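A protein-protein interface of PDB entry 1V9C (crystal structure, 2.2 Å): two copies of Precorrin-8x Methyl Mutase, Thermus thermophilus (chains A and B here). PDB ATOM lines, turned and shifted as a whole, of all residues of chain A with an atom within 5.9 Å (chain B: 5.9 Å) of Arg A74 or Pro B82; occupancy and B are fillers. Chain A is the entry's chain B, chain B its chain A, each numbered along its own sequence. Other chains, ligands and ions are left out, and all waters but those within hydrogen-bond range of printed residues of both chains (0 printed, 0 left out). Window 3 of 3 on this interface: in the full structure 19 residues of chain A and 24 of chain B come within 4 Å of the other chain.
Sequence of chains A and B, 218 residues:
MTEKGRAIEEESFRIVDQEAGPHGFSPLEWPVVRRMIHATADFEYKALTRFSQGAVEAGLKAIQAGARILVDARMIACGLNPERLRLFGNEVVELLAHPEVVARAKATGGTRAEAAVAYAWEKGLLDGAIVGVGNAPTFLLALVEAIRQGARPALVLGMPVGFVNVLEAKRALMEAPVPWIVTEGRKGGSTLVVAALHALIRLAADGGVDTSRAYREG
The guanidinium group (NE) of Arg A74 is in hydrogen-bond range of the backbone carbonyl oxygen (O) of Cys B78 (2.9 Å). SG of Cys B78 forms a disulfide with SG of Cys A78 (2.0 Å). The side-chain amide oxygen of Asn B81 sits close to the guanidinium group of Arg A74 (3.1 Å).
The backbone carbonyl oxygen of Gly B79 lies close to a ring nitrogen (NE2) of His B198, 3.3 Å away. N of Asn B81 sits at hydrogen-bond distance from NE2 of His B198 (3.0 Å).
Among the printed residues, merely in contact across the chains: Arg A74 with Pro B82 (3.8 Å) and Met A75 with Gly B79 (3.4 Å).
Of chain A, only Arg A74 (3.8 Å) comes within 4 Å of Pro B82. Printed residues of chain A within 4 Å of Asn B81: Arg A74 (3.0 Å). Of the printed residues of chain A, Gly B79 touches Met A75 (3.4 Å). Ala A73 touches none of the printed residues of chain B. Leu B87 touches none of the printed residues of chain A. The nearest residue of chain B that does not touch Arg A74 is Gly B79 (4.03 Å). The nearest printed residue of chain A that does not touch Pro B82 is Ala A97 (8.4 Å).
Printed residues of chain B that touch a printed residue of chain A: Cys B78, Gly B79, Asn B81 and Pro B82. Hydrophobic or aromatic side chains of chain B within 4 Å of the printed part of chain A: Pro B82. Of the 11 printed residues of chain A, 3 touch a printed residue of chain B. Hydrophobic or aromatic side chains of chain A within 4 Å of the printed part of chain B: Met A75.
Cys A78 touches its own counterpart, Cys B78. Of the 5 pairs that touch across the chains among the printed residues, 1 has its exchanged pair printed and touching as well.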
ATOM      1  N   VAL A  71     -22.055 -27.853  16.666  1.00  0.00           N
ATOM      2  CA  VAL A  71     -20.865 -28.535  17.117  1.00  0.00           C
ATOM      3  C   VAL A  71     -19.894 -27.609  17.826  1.00  0.00           C
ATOM      4  O   VAL A  71     -19.963 -26.384  17.666  1.00  0.00           O
ATOM      5  CB  VAL A  71     -20.190 -29.262  15.914  1.00  0.00           C
ATOM      6  CG1 VAL A  71     -21.164 -30.250  15.325  1.00  0.00           C
ATOM      7  CG2 VAL A  71     -19.781 -28.264  14.832  1.00  0.00           C
ATOM      8  N   ASP A  72     -18.994 -28.209  18.604  1.00  0.00           N
ATOM      9  CA  ASP A  72     -18.008 -27.465  19.388  1.00  0.00           C
ATOM     10  C   ASP A  72     -16.596 -27.415  18.805  1.00  0.00           C
ATOM     11  O   ASP A  72     -15.639 -27.092  19.520  1.00  0.00           O
ATOM     12  CB  ASP A  72     -17.936 -28.059  20.791  1.00  0.00           C
ATOM     13  CG  ASP A  72     -17.145 -29.350  20.833  1.00  0.00           C
ATOM     14  OD1 ASP A  72     -16.976 -29.979  19.766  1.00  0.00           O
ATOM     15  OD2 ASP A  72     -16.698 -29.739  21.933  1.00  0.00           O
ATOM     16  N   ALA A  73     -16.450 -27.748  17.527  1.00  0.00           N
ATOM     17  CA  ALA A  73     -15.139 -27.710  16.890  1.00  0.00           C
ATOM     18  C   ALA A  73     -15.252 -27.753  15.383  1.00  0.00           C
ATOM     19  O   ALA A  73     -16.092 -28.470  14.827  1.00  0.00           O
ATOM     20  CB  ALA A  73     -14.259 -28.872  17.376  1.00  0.00           C
ATOM     21  N   ARG A  74     -14.390 -26.985  14.725  1.00  0.00           N
ATOM     22  CA  ARG A  74     -14.366 -26.924  13.269  1.00  0.00           C
ATOM     23  C   ARG A  74     -14.060 -28.285  12.640  1.00  0.00           C
ATOM     24  O   ARG A  74     -14.627 -28.627  11.601  1.00  0.00           O
ATOM     25  CB  ARG A  74     -13.342 -25.887  12.819  1.00  0.00           C
ATOM     26  CG  ARG A  74     -12.011 -26.035  13.504  1.00  0.00           C
ATOM     27  CD  ARG A  74     -11.257 -24.721  13.525  1.00  0.00           C
ATOM     28  NE  ARG A  74      -9.976 -24.854  14.211  1.00  0.00           N
ATOM     29  CZ  ARG A  74      -9.312 -23.835  14.744  1.00  0.00           C
ATOM     30  NH1 ARG A  74      -9.810 -22.605  14.669  1.00  0.00           N
ATOM     31  NH2 ARG A  74      -8.155 -24.048  15.353  1.00  0.00           N
ATOM     32  N   MET A  75     -13.188 -29.069  13.278  1.00  0.00           N
ATOM     33  CA  MET A  75     -12.852 -30.397  12.753  1.00  0.00           C
ATOM     34  C   MET A  75     -14.132 -31.195  12.536  1.00  0.00           C
ATOM     35  O   MET A  75     -14.268 -31.914  11.549  1.00  0.00           O
ATOM     36  CB  MET A  75     -11.929 -31.166  13.716  1.00  0.00           C
ATOM     37  CG  MET A  75     -10.481 -30.731  13.651  1.00  0.00           C
ATOM     38  SD  MET A  75      -9.349 -31.891  14.461  1.00  0.00           S
ATOM     39  CE  MET A  75      -9.126 -33.119  13.197  1.00  0.00           C
ATOM     40  N   ILE A  76     -15.063 -31.076  13.473  1.00  0.00           N
ATOM     41  CA  ILE A  76     -16.344 -31.764  13.336  1.00  0.00           C
ATOM     42  C   ILE A  76     -17.124 -31.191  12.151  1.00  0.00           C
ATOM     43  O   ILE A  76     -17.645 -31.937  11.314  1.00  0.00           O
ATOM     44  CB  ILE A  76     -17.191 -31.611  14.623  1.00  0.00           C
ATOM     45  CG1 ILE A  76     -16.512 -32.391  15.756  1.00  0.00           C
ATOM     46  CG2 ILE A  76     -18.621 -32.064  14.390  1.00  0.00           C
ATOM     47  CD1 ILE A  76     -17.230 -32.315  17.079  1.00  0.00           C
ATOM     48  N   ALA A  77     -17.188 -29.861  12.078  1.00  0.00           N
ATOM     49  CA  ALA A  77     -17.903 -29.198  10.998  1.00  0.00           C
ATOM     50  C   ALA A  77     -17.339 -29.627   9.657  1.00  0.00           C
ATOM     51  O   ALA A  77     -18.088 -30.014   8.765  1.00  0.00           O
ATOM     52  CB  ALA A  77     -17.798 -27.689  11.141  1.00  0.00           C
ATOM     53  N   CYS A  78     -16.015 -29.580   9.520  1.00  0.00           N
ATOM     54  CA  CYS A  78     -15.394 -29.948   8.255  1.00  0.00           C
ATOM     55  C   CYS A  78     -15.334 -31.452   8.063  1.00  0.00           C
ATOM     56  O   CYS A  78     -15.393 -31.938   6.936  1.00  0.00           O
ATOM     57  CB  CYS A  78     -13.990 -29.355   8.144  1.00  0.00           C
ATOM     58  SG  CYS A  78     -13.913 -27.533   8.069  1.00  0.00           S
ATOM     59  N   GLY A  79     -15.226 -32.192   9.159  1.00  0.00           N
ATOM     60  CA  GLY A  79     -15.177 -33.634   9.044  1.00  0.00           C
ATOM     61  C   GLY A  79     -16.427 -34.179   8.381  1.00  0.00           C
ATOM     62  O   GLY A  79     -16.372 -35.136   7.612  1.00  0.00           O
ATOM     63  N   GLU A  94     -20.983 -24.205  13.742  1.00  0.00           N
ATOM     64  CA  GLU A  94     -19.828 -24.293  14.619  1.00  0.00           C
ATOM     65  C   GLU A  94     -19.907 -23.106  15.581  1.00  0.00           C
ATOM     66  O   GLU A  94     -19.649 -21.960  15.204  1.00  0.00           O
ATOM     67  CB  GLU A  94     -18.540 -24.252  13.782  1.00  0.00           C
ATOM     68  CG  GLU A  94     -17.288 -23.760  14.515  1.00  0.00           C
ATOM     69  CD  GLU A  94     -16.956 -24.557  15.760  1.00  0.00           C
ATOM     70  OE1 GLU A  94     -15.948 -24.228  16.428  1.00  0.00           O
ATOM     71  OE2 GLU A  94     -17.698 -25.511  16.073  1.00  0.00           O
ATOM     72  N   ALA A  97     -16.169 -21.315  17.486  1.00  0.00           N
ATOM     73  CA  ALA A  97     -15.361 -20.474  16.614  1.00  0.00           C
ATOM     74  C   ALA A  97     -16.241 -19.452  15.906  1.00  0.00           C
ATOM     75  O   ALA A  97     -15.765 -18.699  15.064  1.00  0.00           O
ATOM     76  CB  ALA A  97     -14.626 -21.329  15.591  1.00  0.00           C
ATOM     77  N   CYS B  78      -8.977 -27.795   8.502  1.00  0.00           N
ATOM     78  CA  CYS B  78      -9.714 -26.964   9.444  1.00  0.00           C
ATOM     79  C   CYS B  78      -9.281 -27.197  10.885  1.00  0.00           C
ATOM     80  O   CYS B  78      -9.580 -26.388  11.764  1.00  0.00           O
ATOM     81  CB  CYS B  78     -11.211 -27.240   9.354  1.00  0.00           C
ATOM     82  SG  CYS B  78     -11.942 -27.178   7.685  1.00  0.00           S
ATOM     83  N   GLY B  79      -8.592 -28.306  11.137  1.00  0.00           N
ATOM     84  CA  GLY B  79      -8.159 -28.590  12.491  1.00  0.00           C
ATOM     85  C   GLY B  79      -6.923 -27.806  12.866  1.00  0.00           C
ATOM     86  O   GLY B  79      -6.655 -27.553  14.044  1.00  0.00           O
ATOM     87  N   LEU B  80      -6.159 -27.416  11.856  1.00  0.00           N
ATOM     88  CA  LEU B  80      -4.951 -26.655  12.096  1.00  0.00           C
ATOM     89  C   LEU B  80      -5.297 -25.237  12.519  1.00  0.00           C
ATOM     90  O   LEU B  80      -5.763 -24.433  11.709  1.00  0.00           O
ATOM     91  CB  LEU B  80      -4.088 -26.635  10.834  1.00  0.00           C
ATOM     92  CG  LEU B  80      -3.371 -27.954  10.532  1.00  0.00           C
ATOM     93  CD1 LEU B  80      -2.596 -27.827   9.235  1.00  0.00           C
ATOM     94  CD2 LEU B  80      -2.435 -28.302  11.687  1.00  0.00           C
ATOM     95  N   ASN B  81      -5.073 -24.936  13.794  1.00  0.00           N
ATOM     96  CA  ASN B  81      -5.359 -23.611  14.326  1.00  0.00           C
ATOM     97  C   ASN B  81      -4.595 -22.542  13.532  1.00  0.00           C
ATOM     98  O   ASN B  81      -3.371 -22.458  13.606  1.00  0.00           O
ATOM     99  CB  ASN B  81      -4.977 -23.568  15.810  1.00  0.00           C
ATOM    100  CG  ASN B  81      -5.412 -22.286  16.490  1.00  0.00           C
ATOM    101  OD1 ASN B  81      -6.324 -21.600  16.026  1.00  0.00           O
ATOM    102  ND2 ASN B  81      -4.773 -21.963  17.612  1.00  0.00           N
ATOM    103  N   PRO B  82      -5.318 -21.717  12.751  1.00  0.00           N
ATOM    104  CA  PRO B  82      -4.733 -20.648  11.929  1.00  0.00           C
ATOM    105  C   PRO B  82      -3.829 -19.697  12.709  1.00  0.00           C
ATOM    106  O   PRO B  82      -2.871 -19.145  12.169  1.00  0.00           O
ATOM    107  CB  PRO B  82      -5.962 -19.936  11.367  1.00  0.00           C
ATOM    108  CG  PRO B  82      -6.960 -21.037  11.253  1.00  0.00           C
ATOM    109  CD  PRO B  82      -6.780 -21.762  12.570  1.00  0.00           C
ATOM    110  N   GLU B  83      -4.144 -19.505  13.983  1.00  0.00           N
ATOM    111  CA  GLU B  83      -3.354 -18.621  14.825  1.00  0.00           C
ATOM    112  C   GLU B  83      -1.976 -19.227  15.088  1.00  0.00           C
ATOM    113  O   GLU B  83      -1.099 -18.583  15.668  1.00  0.00           O
ATOM    114  CB  GLU B  83      -4.090 -18.367  16.142  1.00  0.00           C
ATOM    115  CG  GLU B  83      -3.476 -17.276  16.996  1.00  0.00           C
ATOM    116  CD  GLU B  83      -4.383 -16.856  18.136  1.00  0.00           C
ATOM    117  OE1 GLU B  83      -3.981 -15.971  18.923  1.00  0.00           O
ATOM    118  OE2 GLU B  83      -5.500 -17.410  18.242  1.00  0.00           O
ATOM    119  N   ARG B  84      -1.788 -20.471  14.656  1.00  0.00           N
ATOM    120  CA  ARG B  84      -0.513 -21.159  14.834  1.00  0.00           C
ATOM    121  C   ARG B  84       0.192 -21.292  13.488  1.00  0.00           C
ATOM    122  O   ARG B  84       1.419 -21.275  13.411  1.00  0.00           O
ATOM    123  CB  ARG B  84      -0.728 -22.553  15.441  1.00  0.00           C
ATOM    124  CG  ARG B  84      -1.490 -22.560  16.753  1.00  0.00           C
ATOM    125  CD  ARG B  84      -0.859 -21.616  17.760  1.00  0.00           C
ATOM    126  NE  ARG B  84      -1.580 -21.599  19.027  1.00  0.00           N
ATOM    127  CZ  ARG B  84      -1.313 -20.760  20.024  1.00  0.00           C
ATOM    128  NH1 ARG B  84      -0.341 -19.864  19.899  1.00  0.00           N
ATOM    129  NH2 ARG B  84      -2.016 -20.818  21.150  1.00  0.00           N
ATOM    130  N   LEU B  85      -0.600 -21.417  12.429  1.00  0.00           N
ATOM    131  CA  LEU B  85      -0.075 -21.558  11.076  1.00  0.00           C
ATOM    132  C   LEU B  85       0.600 -20.274  10.605  1.00  0.00           C
ATOM    133  O   LEU B  85       1.582 -20.306   9.864  1.00  0.00           O
ATOM    134  CB  LEU B  85      -1.213 -21.912  10.123  1.00  0.00           C
ATOM    135  CG  LEU B  85      -1.083 -23.201   9.314  1.00  0.00           C
ATOM    136  CD1 LEU B  85      -0.828 -24.376  10.240  1.00  0.00           C
ATOM    137  CD2 LEU B  85      -2.353 -23.408   8.516  1.00  0.00           C
ATOM    138  N   ARG B  86       0.055 -19.146  11.048  1.00  0.00           N
ATOM    139  CA  ARG B  86       0.555 -17.826  10.690  1.00  0.00           C
ATOM    140  C   ARG B  86       1.945 -17.523  11.250  1.00  0.00           C
ATOM    141  O   ARG B  86       2.736 -16.841  10.600  1.00  0.00           O
ATOM    142  CB  ARG B  86      -0.450 -16.768  11.160  1.00  0.00           C
ATOM    143  CG  ARG B  86      -0.032 -15.318  10.941  1.00  0.00           C
ATOM    144  CD  ARG B  86      -1.220 -14.380  11.155  1.00  0.00           C
ATOM    145  NE  ARG B  86      -1.941 -14.671  12.393  1.00  0.00           N
ATOM    146  CZ  ARG B  86      -1.430 -14.524  13.611  1.00  0.00           C
ATOM    147  NH1 ARG B  86      -0.189 -14.085  13.764  1.00  0.00           N
ATOM    148  NH2 ARG B  86      -2.161 -14.820  14.678  1.00  0.00           N
ATOM    149  N   LEU B  87       2.239 -18.031  12.445  1.00  0.00           N
ATOM    150  CA  LEU B  87       3.536 -17.803  13.084  1.00  0.00           C
ATOM    151  C   LEU B  87       4.680 -17.855  12.076  1.00  0.00           C
ATOM    152  O   LEU B  87       5.512 -16.949  12.019  1.00  0.00           O
ATOM    153  CB  LEU B  87       3.784 -18.838  14.182  1.00  0.00           C
ATOM    154  CG  LEU B  87       2.809 -18.887  15.359  1.00  0.00           C
ATOM    155  CD1 LEU B  87       3.261 -19.959  16.341  1.00  0.00           C
ATOM    156  CD2 LEU B  87       2.742 -17.528  16.042  1.00  0.00           C
ATOM    157  N   HIS B 198       0.381 -29.561  15.500  1.00  0.00           N
ATOM    158  CA  HIS B 198       0.323 -28.508  16.506  1.00  0.00           C
ATOM    159  C   HIS B 198       1.518 -28.634  17.445  1.00  0.00           C
ATOM    160  O   HIS B 198       1.964 -27.650  18.005  1.00  0.00           O
ATOM    161  CB  HIS B 198      -0.960 -28.608  17.330  1.00  0.00           C
ATOM    162  CG  HIS B 198      -2.174 -28.111  16.618  1.00  0.00           C
ATOM    163  ND1 HIS B 198      -3.444 -28.548  16.925  1.00  0.00           N
ATOM    164  CD2 HIS B 198      -2.316 -27.203  15.625  1.00  0.00           C
ATOM    165  CE1 HIS B 198      -4.318 -27.932  16.150  1.00  0.00           C
ATOM    166  NE2 HIS B 198      -3.660 -27.111  15.352  1.00  0.00           N
